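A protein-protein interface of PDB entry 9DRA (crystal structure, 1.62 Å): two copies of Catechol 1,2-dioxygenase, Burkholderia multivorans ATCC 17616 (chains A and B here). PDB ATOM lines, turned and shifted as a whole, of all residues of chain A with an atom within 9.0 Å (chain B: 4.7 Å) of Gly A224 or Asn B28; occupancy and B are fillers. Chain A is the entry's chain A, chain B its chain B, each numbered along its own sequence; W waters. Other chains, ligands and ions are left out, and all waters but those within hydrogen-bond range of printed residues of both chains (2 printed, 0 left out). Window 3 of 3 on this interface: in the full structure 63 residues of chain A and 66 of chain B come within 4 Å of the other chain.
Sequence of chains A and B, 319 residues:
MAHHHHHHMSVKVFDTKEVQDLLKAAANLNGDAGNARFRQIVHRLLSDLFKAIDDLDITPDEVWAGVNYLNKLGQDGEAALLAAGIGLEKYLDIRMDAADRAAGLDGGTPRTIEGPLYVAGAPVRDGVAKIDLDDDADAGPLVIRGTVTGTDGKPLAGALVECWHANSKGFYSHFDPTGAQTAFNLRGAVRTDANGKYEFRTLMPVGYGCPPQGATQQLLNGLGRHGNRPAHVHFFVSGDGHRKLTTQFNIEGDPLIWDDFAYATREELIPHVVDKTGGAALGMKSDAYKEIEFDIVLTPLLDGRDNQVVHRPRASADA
Gln A218 touches none of the printed residues of chain B. Of the printed residues of chain B, Leu A223 touches Ala B26 (3.3 Å), Ala B27 (3.6 Å), Asn B28 (2.9 Å) and Arg B39 (3.0 Å). Of chain B, only Asn B28 comes within 4 Å of Gly A224. Printed residues of chain B within 4 Å of Tyr A263: Ala B25 (3.3 Å) and Ala B26 (3.3 Å). Printed residues of chain A within 4 Å of Ala B26: Ile A86 (3.4 Å), Leu A223 (3.3 Å), Arg A225 (2.9 Å) and Tyr A263 (3.3 Å). Of the printed residues of chain A, Asn B28 touches Leu A223, Gly A224 and Arg A225.
No position is printed for both chains.
Water W1 lies within hydrogen-bond range of the backbone carbonyl oxygen (O) of Gly A222 (2.8 Å), the guanidinium group (NH2) of Arg B39 (3.0 Å), the backbone carbonyl oxygen (O) of Leu A223 (3.3 Å) and the backbone NH (N) of Gly A224 (3.5 Å). Water W2 bridges ND2 of Asn B28 (3.0 Å) and O of Gly A224 (3.4 Å).
O of Ile A86 touches CB of Ala B26, at 3.4 Å. Ala B26 touches Leu A223. Ala B27 touches Leu A223. O of Gly A224 touches ND2 of Asn B28 (3.6 Å). Arg A225 touches Ala B25. Asn B28 touches Arg A225.
Of the 9 printed residues of chain B, 5 touch a printed residue of chain A. Printed residues of chain B that touch a printed residue of chain A: Ala B25, Ala B26, Ala B27, Asn B28 and Arg B39. Hydrophobic or aromatic side chains of chain B that line the printed part of chain A: Ala B25 and Ala B26. Among the printed residues, no Asp or Glu carboxylate lies within 4 Å of a Lys or Arg side-chain nitrogen of the other chain.
The backbone carbonyl oxygen (O) of Gly A85 lies within hydrogen-bond range of the guanidinium group (NH1) of Arg A225, 2.8 Å away. O of Leu A220 sits at hydrogen-bond distance from N of Arg A225 (2.9 Å). NH2 of Arg A225 sits close to OH of Tyr A263, at 3.2 Å. The side-chain amide oxygen (OD1) of Asn B28 lies close to the backbone NH (N) of Gly B31 (3.5 Å). The backbone carbonyl oxygen of Asn B28 sits at hydrogen-bond distance from the guanidinium group of Arg B39.
The backbone carbonyl oxygen (O) of Leu A223 lies within hydrogen-bond range of the side-chain amide nitrogen (ND2) of Asn B28, 2.9 Å away. O of Leu A223 sits at hydrogen-bond distance from NE of Arg B39, 3.0 Å away. The backbone carbonyl oxygen (O) of Ala B26 is in hydrogen-bond range of the guanidinium group (NH1) of Arg A225, 2.9 Å away. The backbone carbonyl oxygen (O) of Ala B25 is in hydrogen-bond range of the side-chain hydroxyl (OH) of Tyr A263, 3.3 Å away. The backbone NH (N) of Ala B26 sits close to the side-chain hydroxyl (OH) of Tyr A263, 3.4 Å away.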
ATOM      1  N   GLY A  85      25.771  -5.963  22.515  1.00  0.00           N
ATOM      2  CA  GLY A  85      25.679  -7.368  22.867  1.00  0.00           C
ATOM      3  C   GLY A  85      26.400  -7.770  24.142  1.00  0.00           C
ATOM      4  O   GLY A  85      26.016  -8.756  24.778  1.00  0.00           O
ATOM      5  N   ILE A  86      27.475  -7.081  24.513  1.00  0.00           N
ATOM      6  CA  ILE A  86      28.120  -7.383  25.783  1.00  0.00           C
ATOM      7  C   ILE A  86      27.703  -6.391  26.874  1.00  0.00           C
ATOM      8  O   ILE A  86      28.335  -6.325  27.928  1.00  0.00           O
ATOM      9  CB  ILE A  86      29.650  -7.499  25.670  1.00  0.00           C
ATOM     10  CG1 ILE A  86      30.254  -6.401  24.852  1.00  0.00           C
ATOM     11  CG2 ILE A  86      30.015  -8.851  25.076  1.00  0.00           C
ATOM     12  CD1 ILE A  86      30.005  -5.044  25.394  1.00  0.00           C
ATOM     13  N   GLN A 217      28.314 -12.068  16.461  1.00  0.00           N
ATOM     14  CA  GLN A 217      27.834 -13.431  16.673  1.00  0.00           C
ATOM     15  C   GLN A 217      28.971 -14.418  16.868  1.00  0.00           C
ATOM     16  O   GLN A 217      28.797 -15.429  17.550  1.00  0.00           O
ATOM     17  CB  GLN A 217      26.942 -13.880  15.509  1.00  0.00           C
ATOM     18  CG  GLN A 217      26.156 -15.146  15.794  1.00  0.00           C
ATOM     19  CD  GLN A 217      25.203 -14.985  16.972  1.00  0.00           C
ATOM     20  OE1 GLN A 217      24.361 -14.090  16.976  1.00  0.00           O
ATOM     21  NE2 GLN A 217      25.377 -15.812  18.004  1.00  0.00           N
ATOM     22  N   GLN A 218      30.146 -14.161  16.295  1.00  0.00           N
ATOM     23  CA  GLN A 218      31.255 -15.074  16.543  1.00  0.00           C
ATOM     24  C   GLN A 218      31.627 -15.066  18.023  1.00  0.00           C
ATOM     25  O   GLN A 218      31.773 -16.120  18.650  1.00  0.00           O
ATOM     26  CB  GLN A 218      32.452 -14.702  15.672  1.00  0.00           C
ATOM     27  CG  GLN A 218      33.675 -15.574  15.869  1.00  0.00           C
ATOM     28  CD  GLN A 218      34.822 -15.171  14.945  1.00  0.00           C
ATOM     29  OE1 GLN A 218      34.999 -15.732  13.868  1.00  0.00           O
ATOM     30  NE2 GLN A 218      35.564 -14.171  15.347  1.00  0.00           N
ATOM     31  N   LEU A 219      31.754 -13.873  18.605  1.00  0.00           N
ATOM     32  CA  LEU A 219      32.036 -13.780  20.032  1.00  0.00           C
ATOM     33  C   LEU A 219      30.902 -14.377  20.867  1.00  0.00           C
ATOM     34  O   LEU A 219      31.150 -15.103  21.834  1.00  0.00           O
ATOM     35  CB  LEU A 219      32.291 -12.316  20.397  1.00  0.00           C
ATOM     36  CG  LEU A 219      32.573 -11.992  21.865  1.00  0.00           C
ATOM     37  CD1 LEU A 219      33.534 -10.820  21.972  1.00  0.00           C
ATOM     38  CD2 LEU A 219      31.263 -11.676  22.604  1.00  0.00           C
ATOM     39  N   LEU A 220      29.655 -14.116  20.492  1.00  0.00           N
ATOM     40  CA  LEU A 220      28.535 -14.663  21.259  1.00  0.00           C
ATOM     41  C   LEU A 220      28.538 -16.180  21.199  1.00  0.00           C
ATOM     42  O   LEU A 220      28.309 -16.842  22.212  1.00  0.00           O
ATOM     43  CB  LEU A 220      27.204 -14.103  20.747  1.00  0.00           C
ATOM     44  CG  LEU A 220      27.038 -12.596  20.927  1.00  0.00           C
ATOM     45  CD1 LEU A 220      25.792 -12.063  20.200  1.00  0.00           C
ATOM     46  CD2 LEU A 220      26.956 -12.283  22.414  1.00  0.00           C
ATOM     47  N   ASN A 221      28.832 -16.753  20.022  1.00  0.00           N
ATOM     48  CA  ASN A 221      28.922 -18.205  19.917  1.00  0.00           C
ATOM     49  C   ASN A 221      29.987 -18.741  20.860  1.00  0.00           C
ATOM     50  O   ASN A 221      29.815 -19.802  21.469  1.00  0.00           O
ATOM     51  CB  ASN A 221      29.256 -18.637  18.483  1.00  0.00           C
ATOM     52  CG  ASN A 221      28.117 -18.411  17.506  1.00  0.00           C
ATOM     53  OD1 ASN A 221      26.974 -18.226  17.891  1.00  0.00           O
ATOM     54  ND2 ASN A 221      28.437 -18.462  16.215  1.00  0.00           N
ATOM     55  N   GLY A 222      31.106 -18.023  20.976  1.00  0.00           N
ATOM     56  CA  GLY A 222      32.168 -18.459  21.858  1.00  0.00           C
ATOM     57  C   GLY A 222      31.767 -18.445  23.313  1.00  0.00           C
ATOM     58  O   GLY A 222      32.269 -19.246  24.102  1.00  0.00           O
ATOM     59  N   LEU A 223      30.851 -17.551  23.680  1.00  0.00           N
ATOM     60  CA  LEU A 223      30.311 -17.490  25.029  1.00  0.00           C
ATOM     61  C   LEU A 223      29.142 -18.442  25.247  1.00  0.00           C
ATOM     62  O   LEU A 223      28.749 -18.639  26.391  1.00  0.00           O
ATOM     63  CB  LEU A 223      29.856 -16.067  25.356  1.00  0.00           C
ATOM     64  CG  LEU A 223      30.920 -14.971  25.358  1.00  0.00           C
ATOM     65  CD1 LEU A 223      30.253 -13.627  25.466  1.00  0.00           C
ATOM     66  CD2 LEU A 223      31.920 -15.165  26.528  1.00  0.00           C
ATOM     67  N   GLY A 224      28.585 -19.039  24.186  1.00  0.00           N
ATOM     68  CA  GLY A 224      27.402 -19.862  24.326  1.00  0.00           C
ATOM     69  C   GLY A 224      26.111 -19.079  24.350  1.00  0.00           C
ATOM     70  O   GLY A 224      25.115 -19.555  24.903  1.00  0.00           O
ATOM     71  N   ARG A 225      26.105 -17.877  23.792  1.00  0.00           N
ATOM     72  CA  ARG A 225      24.952 -16.985  23.832  1.00  0.00           C
ATOM     73  C   ARG A 225      24.322 -16.823  22.457  1.00  0.00           C
ATOM     74  O   ARG A 225      25.002 -16.857  21.433  1.00  0.00           O
ATOM     75  CB  ARG A 225      25.354 -15.597  24.351  1.00  0.00           C
ATOM     76  CG  ARG A 225      25.756 -15.551  25.843  1.00  0.00           C
ATOM     77  CD  ARG A 225      26.119 -14.137  26.276  1.00  0.00           C
ATOM     78  NE  ARG A 225      25.067 -13.205  25.911  1.00  0.00           N
ATOM     79  CZ  ARG A 225      25.260 -11.925  25.623  1.00  0.00           C
ATOM     80  NH1 ARG A 225      26.438 -11.351  25.798  1.00  0.00           N
ATOM     81  NH2 ARG A 225      24.271 -11.232  25.057  1.00  0.00           N
ATOM     82  N   HIS A 226      23.010 -16.594  22.437  1.00  0.00           N
ATOM     83  CA  HIS A 226      22.327 -16.214  21.220  1.00  0.00           C
ATOM     84  C   HIS A 226      22.489 -14.718  20.975  1.00  0.00           C
ATOM     85  O   HIS A 226      22.834 -13.948  21.876  1.00  0.00           O
ATOM     86  CB  HIS A 226      20.836 -16.603  21.280  1.00  0.00           C
ATOM     87  CG  HIS A 226      19.990 -15.718  22.151  1.00  0.00           C
ATOM     88  ND1 HIS A 226      19.625 -14.441  21.787  1.00  0.00           N
ATOM     89  CD2 HIS A 226      19.412 -15.943  23.354  1.00  0.00           C
ATOM     90  CE1 HIS A 226      18.875 -13.910  22.740  1.00  0.00           C
ATOM     91  NE2 HIS A 226      18.736 -14.799  23.703  1.00  0.00           N
ATOM     92  N   GLY A 227      22.247 -14.318  19.724  1.00  0.00           N
ATOM     93  CA  GLY A 227      22.351 -12.924  19.317  1.00  0.00           C
ATOM     94  C   GLY A 227      21.047 -12.326  18.816  1.00  0.00           C
ATOM     95  O   GLY A 227      21.040 -11.515  17.887  1.00  0.00           O
ATOM     96  N   ASP A 259      14.763 -12.032  27.278  1.00  0.00           N
ATOM     97  CA  ASP A 259      16.019 -12.679  26.922  1.00  0.00           C
ATOM     98  C   ASP A 259      16.639 -11.982  25.724  1.00  0.00           C
ATOM     99  O   ASP A 259      17.090 -12.625  24.776  1.00  0.00           O
ATOM    100  CB  ASP A 259      15.817 -14.169  26.645  1.00  0.00           C
ATOM    101  CG  ASP A 259      17.130 -14.956  26.674  1.00  0.00           C
ATOM    102  OD1 ASP A 259      18.123 -14.467  27.261  1.00  0.00           O
ATOM    103  OD2 ASP A 259      17.165 -16.067  26.112  1.00  0.00           O
ATOM    104  N   TYR A 263      19.941  -6.635  26.286  1.00  0.00           N
ATOM    105  CA  TYR A 263      19.596  -6.301  27.673  1.00  0.00           C
ATOM    106  C   TYR A 263      18.735  -5.044  27.801  1.00  0.00           C
ATOM    107  O   TYR A 263      18.802  -4.358  28.823  1.00  0.00           O
ATOM    108  CB  TYR A 263      20.867  -6.143  28.514  1.00  0.00           C
ATOM    109  CG  TYR A 263      21.694  -7.400  28.470  1.00  0.00           C
ATOM    110  CD1 TYR A 263      21.262  -8.550  29.078  1.00  0.00           C
ATOM    111  CD2 TYR A 263      22.881  -7.454  27.747  1.00  0.00           C
ATOM    112  CE1 TYR A 263      21.998  -9.719  29.007  1.00  0.00           C
ATOM    113  CE2 TYR A 263      23.605  -8.608  27.671  1.00  0.00           C
ATOM    114  CZ  TYR A 263      23.171  -9.735  28.295  1.00  0.00           C
ATOM    115  OH  TYR A 263      23.908 -10.902  28.226  1.00  0.00           O
ATOM    116  N   LYS B  24      27.818 -10.698  34.631  1.00  0.00           N
ATOM    117  CA  LYS B  24      27.708 -12.158  34.651  1.00  0.00           C
ATOM    118  C   LYS B  24      26.901 -12.669  33.461  1.00  0.00           C
ATOM    119  O   LYS B  24      27.263 -13.670  32.837  1.00  0.00           O
ATOM    120  CB  LYS B  24      27.066 -12.634  35.950  1.00  0.00           C
ATOM    121  CG  LYS B  24      27.965 -12.547  37.163  1.00  0.00           C
ATOM    122  CD  LYS B  24      27.144 -12.736  38.438  1.00  0.00           C
ATOM    123  CE  LYS B  24      28.006 -12.695  39.675  1.00  0.00           C
ATOM    124  NZ  LYS B  24      27.176 -12.777  40.918  1.00  0.00           N
ATOM    125  N   ALA B  25      25.778 -12.016  33.156  1.00  0.00           N
ATOM    126  CA  ALA B  25      24.984 -12.445  32.008  1.00  0.00           C
ATOM    127  C   ALA B  25      25.752 -12.255  30.705  1.00  0.00           C
ATOM    128  O   ALA B  25      25.765 -13.139  29.847  1.00  0.00           O
ATOM    129  CB  ALA B  25      23.668 -11.670  31.969  1.00  0.00           C
ATOM    130  N   ALA B  26      26.399 -11.107  30.539  1.00  0.00           N
ATOM    131  CA  ALA B  26      27.033 -10.810  29.264  1.00  0.00           C
ATOM    132  C   ALA B  26      28.152 -11.794  28.953  1.00  0.00           C
ATOM    133  O   ALA B  26      28.358 -12.154  27.787  1.00  0.00           O
ATOM    134  CB  ALA B  26      27.545  -9.375  29.251  1.00  0.00           C
ATOM    135  N   ALA B  27      28.907 -12.227  29.970  1.00  0.00           N
ATOM    136  CA  ALA B  27      29.964 -13.209  29.761  1.00  0.00           C
ATOM    137  C   ALA B  27      29.439 -14.634  29.885  1.00  0.00           C
ATOM    138  O   ALA B  27      30.201 -15.587  29.696  1.00  0.00           O
ATOM    139  CB  ALA B  27      31.108 -12.965  30.749  1.00  0.00           C
ATOM    140  N   ASN B  28      28.153 -14.787  30.169  1.00  0.00           N
ATOM    141  CA  ASN B  28      27.489 -16.089  30.321  1.00  0.00           C
ATOM    142  C   ASN B  28      28.159 -16.975  31.368  1.00  0.00           C
ATOM    143  O   ASN B  28      28.321 -18.183  31.173  1.00  0.00           O
ATOM    144  CB  ASN B  28      27.405 -16.826  28.987  1.00  0.00           C
ATOM    145  CG  ASN B  28      26.321 -17.859  28.980  1.00  0.00           C
ATOM    146  OD1 ASN B  28      25.356 -17.737  29.728  1.00  0.00           O
ATOM    147  ND2 ASN B  28      26.460 -18.885  28.150  1.00  0.00           N
ATOM    148  N   LEU B  29      28.495 -16.390  32.520  1.00  0.00           N
ATOM    149  CA  LEU B  29      29.180 -17.160  33.554  1.00  0.00           C
ATOM    150  C   LEU B  29      28.308 -18.291  34.075  1.00  0.00           C
ATOM    151  O   LEU B  29      28.805 -19.375  34.395  1.00  0.00           O
ATOM    152  CB  LEU B  29      29.600 -16.252  34.708  1.00  0.00           C
ATOM    153  CG  LEU B  29      30.732 -15.259  34.435  1.00  0.00           C
ATOM    154  CD1 LEU B  29      31.316 -14.754  35.766  1.00  0.00           C
ATOM    155  CD2 LEU B  29      31.844 -15.845  33.580  1.00  0.00           C
ATOM    156  N   ASN B  30      27.006 -18.050  34.195  1.00  0.00           N
ATOM    157  CA  ASN B  30      26.083 -19.050  34.704  1.00  0.00           C
ATOM    158  C   ASN B  30      25.412 -19.836  33.583  1.00  0.00           C
ATOM    159  O   ASN B  30      24.336 -20.405  33.790  1.00  0.00           O
ATOM    160  CB  ASN B  30      25.047 -18.378  35.605  1.00  0.00           C
ATOM    161  CG  ASN B  30      25.694 -17.644  36.779  1.00  0.00           C
ATOM    162  OD1 ASN B  30      26.636 -18.149  37.400  1.00  0.00           O
ATOM    163  ND2 ASN B  30      25.208 -16.441  37.072  1.00  0.00           N
ATOM    164  N   GLY B  31      26.037 -19.889  32.402  1.00  0.00           N
ATOM    165  CA  GLY B  31      25.479 -20.632  31.295  1.00  0.00           C
ATOM    166  C   GLY B  31      25.823 -22.107  31.354  1.00  0.00           C
ATOM    167  O   GLY B  31      26.576 -22.573  32.209  1.00  0.00           O
ATOM    168  N   ARG B  39      35.066 -17.335  28.622  1.00  0.00           N
ATOM    169  CA  ARG B  39      34.118 -16.581  29.431  1.00  0.00           C
ATOM    170  C   ARG B  39      34.826 -15.829  30.555  1.00  0.00           C
ATOM    171  O   ARG B  39      34.479 -14.681  30.858  1.00  0.00           O
ATOM    172  CB  ARG B  39      33.063 -17.519  29.994  1.00  0.00           C
ATOM    173  CG  ARG B  39      32.105 -18.104  28.961  1.00  0.00           C
ATOM    174  CD  ARG B  39      31.235 -19.142  29.623  1.00  0.00           C
ATOM    175  NE  ARG B  39      30.362 -19.799  28.658  1.00  0.00           N
ATOM    176  CZ  ARG B  39      29.557 -20.812  28.937  1.00  0.00           C
ATOM    177  NH1 ARG B  39      29.417 -21.269  30.176  1.00  0.00           N
ATOM    178  NH2 ARG B  39      28.884 -21.394  27.945  1.00  0.00           N
HETATM  179  O   HOH W   1      30.914 -21.085  25.766  1.00  0.00           O
HETATM  180  O   HOH W   2      24.731 -21.315  27.781  1.00  0.00           O
